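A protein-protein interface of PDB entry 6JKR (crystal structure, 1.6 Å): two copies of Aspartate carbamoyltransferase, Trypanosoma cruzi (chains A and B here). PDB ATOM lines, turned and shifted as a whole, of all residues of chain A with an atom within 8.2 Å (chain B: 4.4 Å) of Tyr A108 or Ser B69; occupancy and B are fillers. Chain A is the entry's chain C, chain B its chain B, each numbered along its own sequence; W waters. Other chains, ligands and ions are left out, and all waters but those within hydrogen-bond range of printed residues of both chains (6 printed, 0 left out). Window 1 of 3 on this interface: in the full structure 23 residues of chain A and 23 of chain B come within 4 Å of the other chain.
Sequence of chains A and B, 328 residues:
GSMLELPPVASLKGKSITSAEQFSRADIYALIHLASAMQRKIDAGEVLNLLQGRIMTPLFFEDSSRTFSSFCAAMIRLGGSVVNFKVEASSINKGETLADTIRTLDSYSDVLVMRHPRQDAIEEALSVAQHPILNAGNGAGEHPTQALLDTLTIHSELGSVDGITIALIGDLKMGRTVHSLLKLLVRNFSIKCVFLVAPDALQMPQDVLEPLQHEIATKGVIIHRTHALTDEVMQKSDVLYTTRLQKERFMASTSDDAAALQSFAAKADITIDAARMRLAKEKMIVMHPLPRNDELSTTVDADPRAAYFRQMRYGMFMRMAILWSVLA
Printed residues of chain A that touch a printed residue of chain B: Gly A53, Ile A55, Asn A84, Phe A85, Ser A90, Thr A104, Leu A105, Ser A107, Tyr A108 and Asp A110. Of the 12 printed residues of chain B, 9 touch a printed residue of chain A. Hydrophobic or aromatic side chains of chain B within 4 Å of the printed part of chain A: Phe B68, Ala B73, Met B312 and Met B316. Among the printed residues, 19 pairs touch across the chains. Among the printed residues, Asp or Glu carboxylates within 4 Å of a Lys or Arg side-chain nitrogen of the other chain: Asp A110 with Arg B77.
Printed residues of chain B within 4 Å of Tyr A108: Arg B66 (3.4 Å), Ser B69 (3.7 Å), Ser B70 (3.8 Å), Ala B73 (3.7 Å), Arg B77 (2.8 Å), Met B312 (3.4 Å) and Met B316 (3.9 Å). Ser B69 touches just these residues of chain A: Phe A85 (3.8 Å), Leu A105 (3.6 Å) and Tyr A108 (3.7 Å). Printed residues of chain A within 4 Å of Phe B68: Asn A84. Of the printed residues of chain A, Arg B66 touches Thr A104 (2.9 Å) and Tyr A108 (3.4 Å). His A131 touches none of the printed residues of chain B. The nearest printed residue of chain B that does not touch Tyr A108 is Ser B65 (4.7 Å). The nearest residue of chain A that does not touch Ser B69 is Val A83 (4.3 Å).
Water W4 lies within hydrogen-bond range of the side-chain hydroxyl (OH) of Tyr A108, the backbone carbonyl oxygen (O) of Met B312 and the side-chain hydroxyl (OG) of Ser B70. Water W2 lies within hydrogen-bond range of N of Asn A84 (2.9 Å) and SG of Cys B72 (3.4 Å). Water W5 bridges the backbone carbonyl oxygen (O) of Ser A109 (3.0 Å) and the guanidinium group (NH2) of Arg B77 (3.3 Å).
The guanidinium group of Arg B77 sits at hydrogen-bond distance from the backbone carbonyl oxygen of Gly A53, at 3.2 Å. The side-chain sulfur (SD) of Met B312 sits at hydrogen-bond distance from the side-chain hydroxyl (OG1) of Thr A104 (3.4 Å). The guanidinium group of Arg B66 sits at hydrogen-bond distance from the side-chain hydroxyl of Thr A104, 2.9 Å away. OD2 of Asp A110 lies within salt-bridge range of NH2 of Arg B77, at 2.9 Å. NH2 of Arg B77 sits at hydrogen-bond distance from O of Tyr A108 (2.8 Å).
Arg B77 touches Ile A55. Phe B68 touches Asn A84 (CE2 to O, 3.7 Å). Ser B65 touches Phe A85. Ser B69 touches Phe A85. CB of Ser A90 touches OG of Ser B65 (3.2 Å). OG of Ser A107 touches CB of Met B312 (3.8 Å). Tyr A108 touches Arg B66. CE2 of Tyr A108 touches CB of Ser B69, at 3.7 Å. Tyr A108 touches Met B312 (CE1 to O, 3.4 Å). Tyr A108 touches Met B316 (CD1 to CB, 3.9 Å).
No position is printed for both chains.
O of Ile A55 sits at hydrogen-bond distance from N of Val A111. The backbone carbonyl oxygen (O) of Thr A104 sits close to the side-chain hydroxyl (OG) of Ser A107 (3.4 Å). NH1 of Arg B66 lies close to SD of Met B312, at 3.7 Å. The backbone carbonyl oxygen (O) of Ser B65 is in hydrogen-bond range of the side-chain hydroxyl (OG) of Ser B69 (2.7 Å). SD of Met B316 sits at hydrogen-bond distance from NE of Arg B77, 3.6 Å away. N of Met B316 lies close to OG of Ser B70, at 3.3 Å.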
ATOM      1  N   GLY A  53      21.880  42.358  20.057  1.00  0.00           N
ATOM      2  CA  GLY A  53      23.000  41.616  20.638  1.00  0.00           C
ATOM      3  C   GLY A  53      22.566  40.672  21.747  1.00  0.00           C
ATOM      4  O   GLY A  53      23.416  40.051  22.383  1.00  0.00           O
ATOM      5  N   ARG A  54      21.265  40.547  21.997  1.00  0.00           N
ATOM      6  CA  ARG A  54      20.775  39.605  23.012  1.00  0.00           C
ATOM      7  C   ARG A  54      20.201  38.377  22.317  1.00  0.00           C
ATOM      8  O   ARG A  54      19.594  38.496  21.264  1.00  0.00           O
ATOM      9  CB  ARG A  54      19.686  40.229  23.897  1.00  0.00           C
ATOM     10  CG  ARG A  54      20.056  41.575  24.553  1.00  0.00           C
ATOM     11  CD  ARG A  54      21.324  41.476  25.354  1.00  0.00           C
ATOM     12  NE  ARG A  54      21.128  40.768  26.611  1.00  0.00           N
ATOM     13  CZ  ARG A  54      20.479  41.250  27.667  1.00  0.00           C
ATOM     14  NH1 ARG A  54      20.389  40.508  28.763  1.00  0.00           N
ATOM     15  NH2 ARG A  54      19.897  42.443  27.630  1.00  0.00           N
ATOM     16  N   ILE A  55      20.392  37.211  22.931  1.00  0.00           N
ATOM     17  CA  ILE A  55      19.978  35.935  22.324  1.00  0.00           C
ATOM     18  C   ILE A  55      18.946  35.178  23.162  1.00  0.00           C
ATOM     19  O   ILE A  55      19.092  34.999  24.371  1.00  0.00           O
ATOM     20  CB  ILE A  55      21.219  35.049  22.126  1.00  0.00           C
ATOM     21  CG1 ILE A  55      22.132  35.643  21.046  1.00  0.00           C
ATOM     22  CG2 ILE A  55      20.808  33.592  21.716  1.00  0.00           C
ATOM     23  CD1 ILE A  55      23.447  34.816  20.847  1.00  0.00           C
ATOM     24  N   MET A  56      17.904  34.745  22.473  1.00  0.00           N
ATOM     25  CA  MET A  56      16.940  33.823  23.049  1.00  0.00           C
ATOM     26  C   MET A  56      17.150  32.458  22.402  1.00  0.00           C
ATOM     27  O   MET A  56      17.313  32.346  21.170  1.00  0.00           O
ATOM     28  CB  MET A  56      15.525  34.324  22.792  1.00  0.00           C
ATOM     29  CG  MET A  56      14.436  33.541  23.505  1.00  0.00           C
ATOM     30  SD  MET A  56      13.751  32.289  22.403  1.00  0.00           S
ATOM     31  CE  MET A  56      12.957  33.342  21.173  1.00  0.00           C
ATOM     32  N   THR A  57      17.166  31.417  23.230  1.00  0.00           N
ATOM     33  CA  THR A  57      17.175  30.059  22.686  1.00  0.00           C
ATOM     34  C   THR A  57      15.874  29.384  23.073  1.00  0.00           C
ATOM     35  O   THR A  57      15.584  29.217  24.270  1.00  0.00           O
ATOM     36  CB  THR A  57      18.374  29.228  23.163  1.00  0.00           C
ATOM     37  OG1 THR A  57      19.578  29.853  22.685  1.00  0.00           O
ATOM     38  CG2 THR A  57      18.320  27.827  22.535  1.00  0.00           C
ATOM     39  N   VAL A  82      17.862  34.922  17.751  1.00  0.00           N
ATOM     40  CA  VAL A  82      17.397  33.608  18.185  1.00  0.00           C
ATOM     41  C   VAL A  82      18.421  32.573  17.744  1.00  0.00           C
ATOM     42  O   VAL A  82      18.888  32.619  16.601  1.00  0.00           O
ATOM     43  CB  VAL A  82      16.035  33.281  17.535  1.00  0.00           C
ATOM     44  CG1 VAL A  82      15.586  31.876  17.912  1.00  0.00           C
ATOM     45  CG2 VAL A  82      14.952  34.324  17.976  1.00  0.00           C
ATOM     46  N   VAL A  83      18.822  31.676  18.653  1.00  0.00           N
ATOM     47  CA  VAL A  83      19.610  30.483  18.261  1.00  0.00           C
ATOM     48  C   VAL A  83      18.626  29.352  18.189  1.00  0.00           C
ATOM     49  O   VAL A  83      17.954  29.045  19.175  1.00  0.00           O
ATOM     50  CB  VAL A  83      20.754  30.168  19.224  1.00  0.00           C
ATOM     51  CG1 VAL A  83      21.346  28.783  18.931  1.00  0.00           C
ATOM     52  CG2 VAL A  83      21.795  31.238  19.070  1.00  0.00           C
ATOM     53  N   ASN A  84      18.529  28.788  16.985  1.00  0.00           N
ATOM     54  CA  ASN A  84      17.516  27.781  16.654  1.00  0.00           C
ATOM     55  C   ASN A  84      17.939  26.364  16.977  1.00  0.00           C
ATOM     56  O   ASN A  84      18.137  25.522  16.083  1.00  0.00           O
ATOM     57  CB  ASN A  84      17.111  27.921  15.178  1.00  0.00           C
ATOM     58  CG  ASN A  84      16.296  29.173  14.931  1.00  0.00           C
ATOM     59  OD1 ASN A  84      15.140  29.261  15.357  1.00  0.00           O
ATOM     60  ND2 ASN A  84      16.915  30.177  14.307  1.00  0.00           N
ATOM     61  N   PHE A  85      18.005  26.084  18.265  1.00  0.00           N
ATOM     62  CA  PHE A  85      18.246  24.733  18.790  1.00  0.00           C
ATOM     63  C   PHE A  85      17.065  23.745  18.638  1.00  0.00           C
ATOM     64  O   PHE A  85      15.912  24.074  18.958  1.00  0.00           O
ATOM     65  CB  PHE A  85      18.682  24.873  20.255  1.00  0.00           C
ATOM     66  CG  PHE A  85      19.013  23.574  20.929  1.00  0.00           C
ATOM     67  CD1 PHE A  85      20.274  23.008  20.801  1.00  0.00           C
ATOM     68  CD2 PHE A  85      18.065  22.926  21.696  1.00  0.00           C
ATOM     69  CE1 PHE A  85      20.566  21.812  21.437  1.00  0.00           C
ATOM     70  CE2 PHE A  85      18.357  21.740  22.343  1.00  0.00           C
ATOM     71  CZ  PHE A  85      19.596  21.183  22.211  1.00  0.00           C
ATOM     72  N   LYS A  86      17.369  22.546  18.125  1.00  0.00           N
ATOM     73  CA  LYS A  86      16.408  21.445  17.912  1.00  0.00           C
ATOM     74  C   LYS A  86      16.798  20.228  18.752  1.00  0.00           C
ATOM     75  O   LYS A  86      17.902  19.704  18.634  1.00  0.00           O
ATOM     76  CB  LYS A  86      16.319  21.078  16.413  1.00  0.00           C
ATOM     77  CG  LYS A  86      15.936  19.614  16.081  1.00  0.00           C
ATOM     78  CD  LYS A  86      15.246  19.456  14.715  1.00  0.00           C
ATOM     79  CE  LYS A  86      16.209  19.058  13.603  1.00  0.00           C
ATOM     80  NZ  LYS A  86      15.525  18.251  12.530  1.00  0.00           N
ATOM     81  N   ALA A  89      18.105  17.081  16.847  1.00  0.00           N
ATOM     82  CA  ALA A  89      19.416  17.117  16.181  1.00  0.00           C
ATOM     83  C   ALA A  89      20.557  17.385  17.157  1.00  0.00           C
ATOM     84  O   ALA A  89      21.673  17.738  16.748  1.00  0.00           O
ATOM     85  CB  ALA A  89      19.421  18.193  15.087  1.00  0.00           C
ATOM     86  N   SER A  90      20.275  17.201  18.439  1.00  0.00           N
ATOM     87  CA  SER A  90      21.191  17.599  19.500  1.00  0.00           C
ATOM     88  C   SER A  90      21.890  16.391  20.121  1.00  0.00           C
ATOM     89  O   SER A  90      21.626  15.245  19.742  1.00  0.00           O
ATOM     90  CB  SER A  90      20.406  18.323  20.586  1.00  0.00           C
ATOM     91  OG  SER A  90      19.689  17.412  21.408  1.00  0.00           O
ATOM     92  N   THR A 101      21.962  19.705  28.941  1.00  0.00           N
ATOM     93  CA  THR A 101      21.430  20.459  27.785  1.00  0.00           C
ATOM     94  C   THR A 101      21.122  21.902  28.188  1.00  0.00           C
ATOM     95  O   THR A 101      21.472  22.840  27.480  1.00  0.00           O
ATOM     96  CB  THR A 101      20.155  19.787  27.240  1.00  0.00           C
ATOM     97  OG1 THR A 101      20.522  18.499  26.744  1.00  0.00           O
ATOM     98  CG2 THR A 101      19.546  20.594  26.064  1.00  0.00           C
ATOM     99  N   ILE A 102      20.488  22.074  29.348  1.00  0.00           N
ATOM    100  CA  ILE A 102      20.212  23.423  29.865  1.00  0.00           C
ATOM    101  C   ILE A 102      21.509  24.206  30.090  1.00  0.00           C
ATOM    102  O   ILE A 102      21.632  25.367  29.669  1.00  0.00           O
ATOM    103  CB  ILE A 102      19.393  23.398  31.152  1.00  0.00           C
ATOM    104  CG1 ILE A 102      18.034  22.712  30.932  1.00  0.00           C
ATOM    105  CG2 ILE A 102      19.240  24.830  31.727  1.00  0.00           C
ATOM    106  CD1 ILE A 102      17.198  23.323  29.838  1.00  0.00           C
ATOM    107  N   ARG A 103      22.473  23.594  30.781  1.00  0.00           N
ATOM    108  CA  ARG A 103      23.782  24.220  30.986  1.00  0.00           C
ATOM    109  C   ARG A 103      24.442  24.632  29.665  1.00  0.00           C
ATOM    110  O   ARG A 103      25.052  25.695  29.561  1.00  0.00           O
ATOM    111  CB  ARG A 103      24.717  23.267  31.712  1.00  0.00           C
ATOM    112  CG  ARG A 103      24.262  22.906  33.109  1.00  0.00           C
ATOM    113  CD  ARG A 103      25.299  22.001  33.695  1.00  0.00           C
ATOM    114  NE  ARG A 103      25.110  21.804  35.121  1.00  0.00           N
ATOM    115  CZ  ARG A 103      24.719  20.659  35.663  1.00  0.00           C
ATOM    116  NH1 ARG A 103      24.590  20.589  36.982  1.00  0.00           N
ATOM    117  NH2 ARG A 103      24.453  19.595  34.888  1.00  0.00           N
ATOM    118  N   THR A 104      24.306  23.793  28.654  1.00  0.00           N
ATOM    119  CA  THR A 104      24.873  24.072  27.339  1.00  0.00           C
ATOM    120  C   THR A 104      24.247  25.333  26.740  1.00  0.00           C
ATOM    121  O   THR A 104      24.959  26.300  26.430  1.00  0.00           O
ATOM    122  CB  THR A 104      24.676  22.872  26.393  1.00  0.00           C
ATOM    123  OG1 THR A 104      25.358  21.742  26.974  1.00  0.00           O
ATOM    124  CG2 THR A 104      25.247  23.202  25.000  1.00  0.00           C
ATOM    125  N   LEU A 105      22.922  25.347  26.595  1.00  0.00           N
ATOM    126  CA  LEU A 105      22.302  26.538  25.959  1.00  0.00           C
ATOM    127  C   LEU A 105      22.433  27.797  26.837  1.00  0.00           C
ATOM    128  O   LEU A 105      22.544  28.913  26.333  1.00  0.00           O
ATOM    129  CB  LEU A 105      20.861  26.256  25.474  1.00  0.00           C
ATOM    130  CG  LEU A 105      20.765  25.424  24.151  1.00  0.00           C
ATOM    131  CD1 LEU A 105      21.561  26.018  22.986  1.00  0.00           C
ATOM    132  CD2 LEU A 105      21.205  23.996  24.343  1.00  0.00           C
ATOM    133  N   ASP A 106      22.440  27.623  28.157  1.00  0.00           N
ATOM    134  CA  ASP A 106      22.662  28.727  29.095  1.00  0.00           C
ATOM    135  C   ASP A 106      24.050  29.361  28.901  1.00  0.00           C
ATOM    136  O   ASP A 106      24.270  30.513  29.279  1.00  0.00           O
ATOM    137  CB  ASP A 106      22.546  28.160  30.509  1.00  0.00           C
ATOM    138  CG  ASP A 106      22.484  29.230  31.568  1.00  0.00           C
ATOM    139  OD1 ASP A 106      21.630  30.133  31.448  1.00  0.00           O
ATOM    140  OD2 ASP A 106      23.285  29.120  32.533  1.00  0.00           O
ATOM    141  N   SER A 107      24.985  28.626  28.299  1.00  0.00           N
ATOM    142  CA  SER A 107      26.317  29.149  28.078  1.00  0.00           C
ATOM    143  C   SER A 107      26.379  30.217  27.009  1.00  0.00           C
ATOM    144  O   SER A 107      27.380  30.936  26.939  1.00  0.00           O
ATOM    145  CB  SER A 107      27.278  28.017  27.658  1.00  0.00           C
ATOM    146  OG  SER A 107      27.354  27.038  28.709  1.00  0.00           O
ATOM    147  N   TYR A 108      25.350  30.276  26.161  1.00  0.00           N
ATOM    148  CA  TYR A 108      25.374  31.112  24.946  1.00  0.00           C
ATOM    149  C   TYR A 108      24.315  32.172  24.918  1.00  0.00           C
ATOM    150  O   TYR A 108      24.416  33.093  24.116  1.00  0.00           O
ATOM    151  CB  TYR A 108      25.169  30.253  23.685  1.00  0.00           C
ATOM    152  CG  TYR A 108      26.034  29.014  23.662  1.00  0.00           C
ATOM    153  CD1 TYR A 108      27.405  29.100  23.895  1.00  0.00           C
ATOM    154  CD2 TYR A 108      25.475  27.754  23.430  1.00  0.00           C
ATOM    155  CE1 TYR A 108      28.232  27.918  23.872  1.00  0.00           C
ATOM    156  CE2 TYR A 108      26.270  26.601  23.413  1.00  0.00           C
ATOM    157  CZ  TYR A 108      27.621  26.690  23.629  1.00  0.00           C
ATOM    158  OH  TYR A 108      28.376  25.549  23.590  1.00  0.00           O
ATOM    159  N   SER A 109      23.286  32.003  25.751  1.00  0.00           N
ATOM    160  CA  SER A 109      22.008  32.728  25.606  1.00  0.00           C
ATOM    161  C   SER A 109      21.806  33.738  26.701  1.00  0.00           C
ATOM    162  O   SER A 109      22.404  33.638  27.760  1.00  0.00           O
ATOM    163  CB  SER A 109      20.845  31.743  25.706  1.00  0.00           C
ATOM    164  OG  SER A 109      21.033  30.673  24.812  1.00  0.00           O
ATOM    165  N   ASP A 110      20.929  34.689  26.433  1.00  0.00           N
ATOM    166  CA  ASP A 110      20.489  35.648  27.454  1.00  0.00           C
ATOM    167  C   ASP A 110      19.212  35.200  28.132  1.00  0.00           C
ATOM    168  O   ASP A 110      18.959  35.594  29.275  1.00  0.00           O
ATOM    169  CB  ASP A 110      20.329  37.039  26.830  1.00  0.00           C
ATOM    170  CG  ASP A 110      21.654  37.600  26.376  1.00  0.00           C
ATOM    171  OD1 ASP A 110      22.328  38.265  27.213  1.00  0.00           O
ATOM    172  OD2 ASP A 110      22.039  37.388  25.213  1.00  0.00           O
ATOM    173  N   VAL A 111      18.389  34.403  27.430  1.00  0.00           N
ATOM    174  CA  VAL A 111      17.107  33.928  27.952  1.00  0.00           C
ATOM    175  C   VAL A 111      16.801  32.596  27.256  1.00  0.00           C
ATOM    176  O   VAL A 111      17.097  32.423  26.068  1.00  0.00           O
ATOM    177  CB  VAL A 111      15.966  34.968  27.762  1.00  0.00           C
ATOM    178  CG1 VAL A 111      15.738  35.316  26.270  1.00  0.00           C
ATOM    179  CG2 VAL A 111      14.667  34.488  28.443  1.00  0.00           C
ATOM    180  N   LEU A 112      16.232  31.671  28.021  1.00  0.00           N
ATOM    181  CA  LEU A 112      15.814  30.363  27.478  1.00  0.00           C
ATOM    182  C   LEU A 112      14.297  30.314  27.589  1.00  0.00           C
ATOM    183  O   LEU A 112      13.724  30.782  28.587  1.00  0.00           O
ATOM    184  CB  LEU A 112      16.428  29.210  28.260  1.00  0.00           C
ATOM    185  CG  LEU A 112      17.945  29.244  28.453  1.00  0.00           C
ATOM    186  CD1 LEU A 112      18.354  28.012  29.307  1.00  0.00           C
ATOM    187  CD2 LEU A 112      18.651  29.227  27.111  1.00  0.00           C
ATOM    188  N   HIS A 131      20.847  32.136  33.517  1.00  0.00           N
ATOM    189  CA  HIS A 131      20.020  33.130  32.830  1.00  0.00           C
ATOM    190  C   HIS A 131      18.536  32.799  33.029  1.00  0.00           C
ATOM    191  O   HIS A 131      18.182  31.656  33.359  1.00  0.00           O
ATOM    192  CB  HIS A 131      20.359  33.151  31.321  1.00  0.00           C
ATOM    193  CG  HIS A 131      21.783  33.508  31.024  1.00  0.00           C
ATOM    194  ND1 HIS A 131      22.241  34.811  30.973  1.00  0.00           N
ATOM    195  CD2 HIS A 131      22.851  32.723  30.751  1.00  0.00           C
ATOM    196  CE1 HIS A 131      23.538  34.809  30.702  1.00  0.00           C
ATOM    197  NE2 HIS A 131      23.932  33.554  30.571  1.00  0.00           N
ATOM    198  N   SER B  65      25.183  19.673  19.836  1.00  0.00           N
ATOM    199  CA  SER B  65      24.587  20.719  20.686  1.00  0.00           C
ATOM    200  C   SER B  65      25.556  21.900  20.833  1.00  0.00           C
ATOM    201  O   SER B  65      25.220  23.039  20.476  1.00  0.00           O
ATOM    202  CB  SER B  65      24.203  20.226  22.094  1.00  0.00           C
ATOM    203  OG  SER B  65      23.094  19.317  22.088  1.00  0.00           O
ATOM    204  N   ARG B  66      26.769  21.645  21.312  1.00  0.00           N
ATOM    205  CA  ARG B  66      27.712  22.740  21.555  1.00  0.00           C
ATOM    206  C   ARG B  66      28.239  23.392  20.304  1.00  0.00           C
ATOM    207  O   ARG B  66      28.206  24.630  20.179  1.00  0.00           O
ATOM    208  CB  ARG B  66      28.928  22.207  22.330  1.00  0.00           C
ATOM    209  CG  ARG B  66      28.701  22.143  23.839  1.00  0.00           C
ATOM    210  CD  ARG B  66      29.454  20.892  24.396  1.00  0.00           C
ATOM    211  NE  ARG B  66      28.680  19.718  23.951  1.00  0.00           N
ATOM    212  CZ  ARG B  66      27.567  19.278  24.536  1.00  0.00           C
ATOM    213  NH1 ARG B  66      27.140  19.853  25.677  1.00  0.00           N
ATOM    214  NH2 ARG B  66      26.871  18.302  23.974  1.00  0.00           N
ATOM    215  N   THR B  67      28.751  22.592  19.378  1.00  0.00           N
ATOM    216  CA  THR B  67      29.463  23.200  18.252  1.00  0.00           C
ATOM    217  C   THR B  67      28.513  23.990  17.357  1.00  0.00           C
ATOM    218  O   THR B  67      28.787  25.145  17.007  1.00  0.00           O
ATOM    219  CB  THR B  67      30.280  22.134  17.470  1.00  0.00           C
ATOM    220  OG1 THR B  67      31.090  21.412  18.408  1.00  0.00           O
ATOM    221  CG2 THR B  67      31.231  22.791  16.459  1.00  0.00           C
ATOM    222  N   PHE B  68      27.374  23.407  17.042  1.00  0.00           N
ATOM    223  CA  PHE B  68      26.342  24.132  16.299  1.00  0.00           C
ATOM    224  C   PHE B  68      25.902  25.409  17.032  1.00  0.00           C
ATOM    225  O   PHE B  68      25.940  26.519  16.472  1.00  0.00           O
ATOM    226  CB  PHE B  68      25.133  23.224  16.052  1.00  0.00           C
ATOM    227  CG  PHE B  68      23.923  23.964  15.544  1.00  0.00           C
ATOM    228  CD1 PHE B  68      23.726  24.138  14.170  1.00  0.00           C
ATOM    229  CD2 PHE B  68      22.971  24.465  16.416  1.00  0.00           C
ATOM    230  CE1 PHE B  68      22.601  24.815  13.695  1.00  0.00           C
ATOM    231  CE2 PHE B  68      21.824  25.179  15.929  1.00  0.00           C
ATOM    232  CZ  PHE B  68      21.663  25.348  14.578  1.00  0.00           C
ATOM    233  N   SER B  69      25.496  25.277  18.300  1.00  0.00           N
ATOM    234  CA  SER B  69      24.937  26.442  18.994  1.00  0.00           C
ATOM    235  C   SER B  69      25.953  27.531  19.242  1.00  0.00           C
ATOM    236  O   SER B  69      25.616  28.716  19.119  1.00  0.00           O
ATOM    237  CB  SER B  69      24.322  26.030  20.330  1.00  0.00           C
ATOM    238  OG  SER B  69      23.394  24.981  20.075  1.00  0.00           O
ATOM    239  N   SER B  70      27.181  27.119  19.596  1.00  0.00           N
ATOM    240  CA  SER B  70      28.292  28.044  19.889  1.00  0.00           C
ATOM    241  C   SER B  70      28.642  28.861  18.653  1.00  0.00           C
ATOM    242  O   SER B  70      28.823  30.072  18.726  1.00  0.00           O
ATOM    243  CB  SER B  70      29.511  27.254  20.382  1.00  0.00           C
ATOM    244  OG  SER B  70      30.559  28.103  20.799  1.00  0.00           O
ATOM    245  N   PHE B  71      28.726  28.206  17.499  1.00  0.00           N
ATOM    246  CA  PHE B  71      29.021  28.936  16.251  1.00  0.00           C
ATOM    247  C   PHE B  71      27.892  29.895  15.865  1.00  0.00           C
ATOM    248  O   PHE B  71      28.188  31.028  15.458  1.00  0.00           O
ATOM    249  CB  PHE B  71      29.291  28.010  15.077  1.00  0.00           C
ATOM    250  CG  PHE B  71      30.754  27.672  14.887  1.00  0.00           C
ATOM    251  CD1 PHE B  71      31.664  28.647  14.483  1.00  0.00           C
ATOM    252  CD2 PHE B  71      31.194  26.359  15.062  1.00  0.00           C
ATOM    253  CE1 PHE B  71      33.003  28.316  14.263  1.00  0.00           C
ATOM    254  CE2 PHE B  71      32.550  26.015  14.851  1.00  0.00           C
ATOM    255  CZ  PHE B  71      33.448  27.002  14.444  1.00  0.00           C
ATOM    256  N   CYS B  72      26.636  29.476  16.001  1.00  0.00           N
ATOM    257  CA  CYS B  72      25.482  30.374  15.691  1.00  0.00           C
ATOM    258  C   CYS B  72      25.528  31.570  16.616  1.00  0.00           C
ATOM    259  O   CYS B  72      25.459  32.697  16.140  1.00  0.00           O
ATOM    260  CB  CYS B  72      24.163  29.623  15.862  1.00  0.00           C
ATOM    261  SG  CYS B  72      23.871  28.437  14.564  1.00  0.00           S
ATOM    262  N   ALA B  73      25.664  31.329  17.925  1.00  0.00           N
ATOM    263  CA  ALA B  73      25.730  32.400  18.919  1.00  0.00           C
ATOM    264  C   ALA B  73      26.901  33.328  18.634  1.00  0.00           C
ATOM    265  O   ALA B  73      26.741  34.563  18.689  1.00  0.00           O
ATOM    266  CB  ALA B  73      25.822  31.818  20.350  1.00  0.00           C
ATOM    267  N   ARG B  77      26.636  37.284  17.827  1.00  0.00           N
ATOM    268  CA  ARG B  77      27.228  38.278  18.748  1.00  0.00           C
ATOM    269  C   ARG B  77      28.266  39.123  18.049  1.00  0.00           C
ATOM    270  O   ARG B  77      28.672  40.151  18.601  1.00  0.00           O
ATOM    271  CB  ARG B  77      27.783  37.622  20.015  1.00  0.00           C
ATOM    272  CG  ARG B  77      26.691  37.054  20.921  1.00  0.00           C
ATOM    273  CD  ARG B  77      27.270  36.506  22.206  1.00  0.00           C
ATOM    274  NE  ARG B  77      26.207  35.889  23.017  1.00  0.00           N
ATOM    275  CZ  ARG B  77      25.336  36.574  23.751  1.00  0.00           C
ATOM    276  NH1 ARG B  77      25.399  37.909  23.804  1.00  0.00           N
ATOM    277  NH2 ARG B  77      24.417  35.916  24.464  1.00  0.00           N
ATOM    278  N   MET B 312      32.542  25.458  27.771  1.00  0.00           N
ATOM    279  CA  MET B 312      31.573  25.749  26.704  1.00  0.00           C
ATOM    280  C   MET B 312      31.458  27.248  26.406  1.00  0.00           C
ATOM    281  O   MET B 312      31.355  27.641  25.234  1.00  0.00           O
ATOM    282  CB  MET B 312      30.202  25.149  27.043  1.00  0.00           C
ATOM    283  CG  MET B 312      30.169  23.608  27.037  1.00  0.00           C
ATOM    284  SD  MET B 312      28.462  23.018  27.155  1.00  0.00           S
ATOM    285  CE  MET B 312      28.146  23.148  28.958  1.00  0.00           C
ATOM    286  N   MET B 316      32.388  29.773  22.930  1.00  0.00           N
ATOM    287  CA  MET B 316      31.685  30.812  22.192  1.00  0.00           C
ATOM    288  C   MET B 316      32.630  31.963  21.873  1.00  0.00           C
ATOM    289  O   MET B 316      32.626  32.451  20.739  1.00  0.00           O
ATOM    290  CB  MET B 316      30.436  31.303  22.943  1.00  0.00           C
ATOM    291  CG  MET B 316      29.654  32.357  22.129  1.00  0.00           C
ATOM    292  SD  MET B 316      28.206  32.930  23.040  1.00  0.00           S
ATOM    293  CE  MET B 316      28.976  33.790  24.402  1.00  0.00           C
HETATM  294  O   HOH W   1      22.051  18.541  24.313  1.00  0.00           O
HETATM  295  O   HOH W   2      20.545  29.014  14.910  1.00  0.00           O
HETATM  296  O   HOH W   3      24.489  39.379  26.191  1.00  0.00           O
HETATM  297  O   HOH W   4      30.971  25.989  23.086  1.00  0.00           O
HETATM  298  O   HOH W   5      25.198  34.562  27.413  1.00  0.00           O
HETATM  299  O   HOH W   6      26.065  40.407  22.345  1.00  0.00           O
